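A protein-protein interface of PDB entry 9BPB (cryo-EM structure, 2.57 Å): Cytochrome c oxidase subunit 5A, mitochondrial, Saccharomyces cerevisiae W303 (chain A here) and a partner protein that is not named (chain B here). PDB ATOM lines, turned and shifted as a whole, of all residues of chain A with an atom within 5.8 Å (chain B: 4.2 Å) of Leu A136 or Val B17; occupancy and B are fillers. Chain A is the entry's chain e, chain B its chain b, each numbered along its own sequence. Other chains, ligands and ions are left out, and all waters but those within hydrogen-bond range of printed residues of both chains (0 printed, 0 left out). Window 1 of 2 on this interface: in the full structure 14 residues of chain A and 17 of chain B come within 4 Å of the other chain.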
ATOM      1  N   SER A 132      29.440  19.777   2.153  1.00  0.00           N
ATOM      2  CA  SER A 132      28.622  20.177   3.293  1.00  0.00           C
ATOM      3  C   SER A 132      27.338  19.361   3.374  1.00  0.00           C
ATOM      4  O   SER A 132      26.777  19.195   4.462  1.00  0.00           O
ATOM      5  CB  SER A 132      28.296  21.668   3.212  1.00  0.00           C
ATOM      6  OG  SER A 132      29.471  22.455   3.143  1.00  0.00           O
ATOM      7  N   ASP A 133      26.863  18.842   2.241  1.00  0.00           N
ATOM      8  CA  ASP A 133      25.577  18.155   2.217  1.00  0.00           C
ATOM      9  C   ASP A 133      25.664  16.754   2.804  1.00  0.00           C
ATOM     10  O   ASP A 133      24.694  16.280   3.406  1.00  0.00           O
ATOM     11  CB  ASP A 133      25.050  18.091   0.789  1.00  0.00           C
ATOM     12  CG  ASP A 133      24.987  19.447   0.142  1.00  0.00           C
ATOM     13  OD1 ASP A 133      24.948  20.445   0.890  1.00  0.00           O
ATOM     14  OD2 ASP A 133      24.976  19.517  -1.103  1.00  0.00           O
ATOM     15  N   GLU A 134      26.798  16.073   2.627  1.00  0.00           N
ATOM     16  CA  GLU A 134      26.943  14.730   3.178  1.00  0.00           C
ATOM     17  C   GLU A 134      26.836  14.747   4.696  1.00  0.00           C
ATOM     18  O   GLU A 134      26.231  13.851   5.296  1.00  0.00           O
ATOM     19  CB  GLU A 134      28.275  14.127   2.738  1.00  0.00           C
ATOM     20  CG  GLU A 134      28.439  14.034   1.232  1.00  0.00           C
ATOM     21  CD  GLU A 134      29.848  13.659   0.824  1.00  0.00           C
ATOM     22  OE1 GLU A 134      30.619  13.207   1.695  1.00  0.00           O
ATOM     23  OE2 GLU A 134      30.185  13.822  -0.368  1.00  0.00           O
ATOM     24  N   TYR A 135      27.422  15.763   5.334  1.00  0.00           N
ATOM     25  CA  TYR A 135      27.271  15.924   6.775  1.00  0.00           C
ATOM     26  C   TYR A 135      25.813  16.149   7.154  1.00  0.00           C
ATOM     27  O   TYR A 135      25.313  15.546   8.110  1.00  0.00           O
ATOM     28  CB  TYR A 135      28.142  17.086   7.253  1.00  0.00           C
ATOM     29  CG  TYR A 135      28.041  17.381   8.730  1.00  0.00           C
ATOM     30  CD1 TYR A 135      28.625  16.540   9.667  1.00  0.00           C
ATOM     31  CD2 TYR A 135      27.371  18.508   9.188  1.00  0.00           C
ATOM     32  CE1 TYR A 135      28.538  16.809  11.017  1.00  0.00           C
ATOM     33  CE2 TYR A 135      27.277  18.783  10.536  1.00  0.00           C
ATOM     34  CZ  TYR A 135      27.863  17.932  11.446  1.00  0.00           C
ATOM     35  OH  TYR A 135      27.772  18.204  12.791  1.00  0.00           O
ATOM     36  N   LEU A 136      25.113  17.011   6.410  1.00  0.00           N
ATOM     37  CA  LEU A 136      23.715  17.292   6.717  1.00  0.00           C
ATOM     38  C   LEU A 136      22.823  16.095   6.409  1.00  0.00           C
ATOM     39  O   LEU A 136      21.905  15.786   7.178  1.00  0.00           O
ATOM     40  CB  LEU A 136      23.245  18.520   5.936  1.00  0.00           C
ATOM     41  CG  LEU A 136      24.061  19.800   6.121  1.00  0.00           C
ATOM     42  CD1 LEU A 136      23.473  20.931   5.304  1.00  0.00           C
ATOM     43  CD2 LEU A 136      24.136  20.183   7.590  1.00  0.00           C
ATOM     44  N   LYS A 137      23.073  15.413   5.289  1.00  0.00           N
ATOM     45  CA  LYS A 137      22.227  14.289   4.901  1.00  0.00           C
ATOM     46  C   LYS A 137      22.348  13.135   5.887  1.00  0.00           C
ATOM     47  O   LYS A 137      21.369  12.421   6.138  1.00  0.00           O
ATOM     48  CB  LYS A 137      22.587  13.830   3.486  1.00  0.00           C
ATOM     49  CG  LYS A 137      21.703  12.722   2.942  1.00  0.00           C
ATOM     50  CD  LYS A 137      22.024  12.429   1.488  1.00  0.00           C
ATOM     51  CE  LYS A 137      22.111  10.934   1.231  1.00  0.00           C
ATOM     52  NZ  LYS A 137      20.810  10.371   0.781  1.00  0.00           N
ATOM     53  N   SER A 138      23.538  12.934   6.458  1.00  0.00           N
ATOM     54  CA  SER A 138      23.713  11.869   7.437  1.00  0.00           C
ATOM     55  C   SER A 138      23.001  12.184   8.747  1.00  0.00           C
ATOM     56  O   SER A 138      22.641  11.265   9.491  1.00  0.00           O
ATOM     57  CB  SER A 138      25.200  11.625   7.688  1.00  0.00           C
ATOM     58  OG  SER A 138      25.750  12.637   8.509  1.00  0.00           O
ATOM     59  N   LYS A 139      22.795  13.463   9.047  1.00  0.00           N
ATOM     60  CA  LYS A 139      22.103  13.883  10.257  1.00  0.00           C
ATOM     61  C   LYS A 139      20.625  14.164  10.033  1.00  0.00           C
ATOM     62  O   LYS A 139      19.938  14.550  10.984  1.00  0.00           O
ATOM     63  CB  LYS A 139      22.778  15.127  10.846  1.00  0.00           C
ATOM     64  CG  LYS A 139      24.228  14.920  11.253  1.00  0.00           C
ATOM     65  CD  LYS A 139      24.393  13.660  12.091  1.00  0.00           C
ATOM     66  CE  LYS A 139      25.853  13.262  12.210  1.00  0.00           C
ATOM     67  NZ  LYS A 139      26.610  14.175  13.108  1.00  0.00           N
ATOM     68  N   ASN A 140      20.124  13.984   8.809  1.00  0.00           N
ATOM     69  CA  ASN A 140      18.721  14.232   8.468  1.00  0.00           C
ATOM     70  C   ASN A 140      18.346  15.690   8.743  1.00  0.00           C
ATOM     71  O   ASN A 140      17.475  15.998   9.558  1.00  0.00           O
ATOM     72  CB  ASN A 140      17.799  13.268   9.219  1.00  0.00           C
ATOM     73  CG  ASN A 140      18.209  11.824   9.046  1.00  0.00           C
ATOM     74  OD1 ASN A 140      18.645  11.174   9.994  1.00  0.00           O
ATOM     75  ND2 ASN A 140      18.075  11.313   7.829  1.00  0.00           N
ATOM     76  N   ALA A 141      19.093  16.587   8.113  1.00  0.00           N
ATOM     77  CA  ALA A 141      18.926  18.022   8.399  1.00  0.00           C
ATOM     78  C   ALA A 141      17.494  18.493   8.192  1.00  0.00           C
ATOM     79  O   ALA A 141      16.938  19.066   9.130  1.00  0.00           O
ATOM     80  CB  ALA A 141      19.855  18.794   7.519  1.00  0.00           C
ATOM     81  N   ASN A 142      16.924  18.301   7.009  1.00  0.00           N
ATOM     82  CA  ASN A 142      15.601  18.865   6.769  1.00  0.00           C
ATOM     83  C   ASN A 142      14.679  17.830   6.132  1.00  0.00           C
ATOM     84  O   ASN A 142      14.849  17.487   4.955  1.00  0.00           O
ATOM     85  CB  ASN A 142      15.703  20.110   5.884  1.00  0.00           C
ATOM     86  CG  ASN A 142      16.135  21.345   6.659  1.00  0.00           C
ATOM     87  OD1 ASN A 142      15.659  21.596   7.764  1.00  0.00           O
ATOM     88  ND2 ASN A 142      17.034  22.127   6.073  1.00  0.00           N
ATOM     89  N   TYR A 147      18.381  20.754   2.192  1.00  0.00           N
ATOM     90  CA  TYR A 147      19.643  21.131   2.815  1.00  0.00           C
ATOM     91  C   TYR A 147      20.728  21.228   1.753  1.00  0.00           C
ATOM     92  O   TYR A 147      21.864  20.791   1.955  1.00  0.00           O
ATOM     93  CB  TYR A 147      20.027  20.130   3.897  1.00  0.00           C
ATOM     94  CG  TYR A 147      19.710  18.702   3.517  1.00  0.00           C
ATOM     95  CD1 TYR A 147      20.578  17.967   2.718  1.00  0.00           C
ATOM     96  CD2 TYR A 147      18.540  18.093   3.947  1.00  0.00           C
ATOM     97  CE1 TYR A 147      20.289  16.664   2.363  1.00  0.00           C
ATOM     98  CE2 TYR A 147      18.243  16.789   3.596  1.00  0.00           C
ATOM     99  CZ  TYR A 147      19.122  16.080   2.805  1.00  0.00           C
ATOM    100  OH  TYR A 147      18.828  14.782   2.456  1.00  0.00           O
ATOM    101  N   SER A 148      20.381  21.807   0.600  1.00  0.00           N
ATOM    102  CA  SER A 148      21.226  21.697  -0.585  1.00  0.00           C
ATOM    103  C   SER A 148      22.562  22.409  -0.404  1.00  0.00           C
ATOM    104  O   SER A 148      23.597  21.915  -0.862  1.00  0.00           O
ATOM    105  CB  SER A 148      20.492  22.250  -1.804  1.00  0.00           C
ATOM    106  OG  SER A 148      21.276  22.100  -2.976  1.00  0.00           O
ATOM    107  N   GLN A 149      22.554  23.588   0.217  1.00  0.00           N
ATOM    108  CA  GLN A 149      23.779  24.330   0.532  1.00  0.00           C
ATOM    109  C   GLN A 149      24.632  24.611  -0.704  1.00  0.00           C
ATOM    110  O   GLN A 149      25.843  24.809  -0.594  1.00  0.00           O
ATOM    111  CB  GLN A 149      24.616  23.593   1.584  1.00  0.00           C
ATOM    112  CG  GLN A 149      24.224  23.881   3.023  1.00  0.00           C
ATOM    113  CD  GLN A 149      24.006  25.355   3.283  1.00  0.00           C
ATOM    114  OE1 GLN A 149      22.931  25.765   3.712  1.00  0.00           O
ATOM    115  NE2 GLN A 149      25.029  26.162   3.026  1.00  0.00           N
ATOM    116  N   ASP B  16      17.493  23.669  12.208  1.00  0.00           N
ATOM    117  CA  ASP B  16      18.589  23.114  11.381  1.00  0.00           C
ATOM    118  C   ASP B  16      19.356  24.265  10.724  1.00  0.00           C
ATOM    119  O   ASP B  16      19.237  25.399  11.199  1.00  0.00           O
ATOM    120  CB  ASP B  16      17.983  22.091  10.428  1.00  0.00           C
ATOM    121  CG  ASP B  16      17.089  21.101  11.149  1.00  0.00           C
ATOM    122  OD1 ASP B  16      17.634  20.247  11.870  1.00  0.00           O
ATOM    123  OD2 ASP B  16      15.857  21.208  11.003  1.00  0.00           O
ATOM    124  N   VAL B  17      20.123  23.985   9.679  1.00  0.00           N
ATOM    125  CA  VAL B  17      20.937  24.974   8.976  1.00  0.00           C
ATOM    126  C   VAL B  17      20.046  25.898   8.157  1.00  0.00           C
ATOM    127  O   VAL B  17      18.977  25.478   7.694  1.00  0.00           O
ATOM    128  CB  VAL B  17      21.979  24.291   8.078  1.00  0.00           C
ATOM    129  CG1 VAL B  17      23.059  23.643   8.921  1.00  0.00           C
ATOM    130  CG2 VAL B  17      21.307  23.263   7.182  1.00  0.00           C
ATOM    131  N   PRO B  18      20.431  27.156   7.966  1.00  0.00           N
ATOM    132  CA  PRO B  18      19.738  27.993   6.983  1.00  0.00           C
ATOM    133  C   PRO B  18      20.090  27.567   5.567  1.00  0.00           C
ATOM    134  O   PRO B  18      21.153  27.001   5.311  1.00  0.00           O
ATOM    135  CB  PRO B  18      20.255  29.403   7.288  1.00  0.00           C
ATOM    136  CG  PRO B  18      21.575  29.180   7.935  1.00  0.00           C
ATOM    137  CD  PRO B  18      21.455  27.906   8.711  1.00  0.00           C
ATOM    138  N   THR B  19      19.178  27.853   4.644  1.00  0.00           N
ATOM    139  CA  THR B  19      19.302  27.475   3.246  1.00  0.00           C
ATOM    140  C   THR B  19      19.504  28.713   2.380  1.00  0.00           C
ATOM    141  O   THR B  19      18.897  29.754   2.647  1.00  0.00           O
ATOM    142  CB  THR B  19      18.045  26.727   2.779  1.00  0.00           C
ATOM    143  OG1 THR B  19      17.692  25.734   3.752  1.00  0.00           O
ATOM    144  CG2 THR B  19      18.270  26.048   1.441  1.00  0.00           C
ATOM    145  N   GLN B  26      12.780  27.691   9.485  1.00  0.00           N
ATOM    146  CA  GLN B  26      13.490  26.425   9.532  1.00  0.00           C
ATOM    147  C   GLN B  26      12.562  25.342  10.068  1.00  0.00           C
ATOM    148  O   GLN B  26      11.636  25.616  10.836  1.00  0.00           O
ATOM    149  CB  GLN B  26      14.735  26.535  10.408  1.00  0.00           C
ATOM    150  CG  GLN B  26      15.811  27.428   9.840  1.00  0.00           C
ATOM    151  CD  GLN B  26      17.013  27.517  10.746  1.00  0.00           C
ATOM    152  OE1 GLN B  26      17.730  28.517  10.753  1.00  0.00           O
ATOM    153  NE2 GLN B  26      17.238  26.472  11.527  1.00  0.00           N
ATOM    154  N   LEU B 158      31.142  23.947   8.001  1.00  0.00           N
ATOM    155  CA  LEU B 158      30.322  25.129   7.760  1.00  0.00           C
ATOM    156  C   LEU B 158      30.972  26.357   8.380  1.00  0.00           C
ATOM    157  O   LEU B 158      31.404  26.326   9.536  1.00  0.00           O
ATOM    158  CB  LEU B 158      28.916  24.931   8.325  1.00  0.00           C
ATOM    159  CG  LEU B 158      27.981  23.999   7.550  1.00  0.00           C
ATOM    160  CD1 LEU B 158      28.189  22.545   7.947  1.00  0.00           C
ATOM    161  CD2 LEU B 158      26.541  24.416   7.759  1.00  0.00           C
ATOM    162  N   TYR B 218      21.608  24.770  14.992  1.00  0.00           N
ATOM    163  CA  TYR B 218      22.829  25.568  14.997  1.00  0.00           C
ATOM    164  C   TYR B 218      22.716  26.925  15.675  1.00  0.00           C
ATOM    165  O   TYR B 218      23.678  27.356  16.312  1.00  0.00           O
ATOM    166  CB  TYR B 218      23.329  25.755  13.563  1.00  0.00           C
ATOM    167  CG  TYR B 218      24.338  24.700  13.183  1.00  0.00           C
ATOM    168  CD1 TYR B 218      25.602  24.690  13.749  1.00  0.00           C
ATOM    169  CD2 TYR B 218      24.019  23.704  12.273  1.00  0.00           C
ATOM    170  CE1 TYR B 218      26.525  23.724  13.411  1.00  0.00           C
ATOM    171  CE2 TYR B 218      24.934  22.734  11.930  1.00  0.00           C
ATOM    172  CZ  TYR B 218      26.186  22.750  12.500  1.00  0.00           C
ATOM    173  OH  TYR B 218      27.104  21.785  12.158  1.00  0.00           O
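The backbone carbonyl oxygen of Pro B18 lies close to the side-chain amide oxygen of Gln A149 (2.7 Å).
O of Ala A141 lies close to OD2 of Asp B16, 3.0 Å away.
OD2 of Asp B16 lies close to OD1 of Asn A142.
N of Ala A141 is in hydrogen-bond range of O of Leu A136, at 3.1 Å.
OG of Ser A138 sits at hydrogen-bond distance from O of Tyr A135.
The backbone NH (N) of Asp B16 sits close to the side-chain amide nitrogen (NE2) of Gln B26.
Tyr A135 touches Tyr B218.
Leu A136 touches Val B17.
Glu A134 touches none of the printed residues of chain B.
Of chain B, only Val B17 (3.7 Å) comes within 4 Å of Leu A136.
Printed residues of chain B within 4 Å of Gln A149: Pro B18 (2.7 Å).
Of the printed residues of chain A, Asp B16 touches Ala A141 and Asn A142.
Val B17 touches one residue of chain A.
Of the printed residues of chain A, Tyr B218 touches Tyr A135.
The nearest residue of chain A that does not touch Val B17 is Asn A142 (4.2 Å).
The nearest printed residue of chain A that does not touch Pro B18 is Asn A142 (6.3 Å).
Hydrophobic or aromatic side chains of chain A that line the printed part of chain B: Tyr A135 and Leu A136.
Along chain A the printed residues that touch a printed residue of chain B span positions 135 to 149.
Printed residues of chain B that touch a printed residue of chain A: Asp B16, Val B17, Pro B18 and Tyr B218.
Hydrophobic or aromatic side chains of chain B within 4 Å of the printed part of chain A: Val B17 and Tyr B218.
Among the printed residues, 5 pairs touch across the chains.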
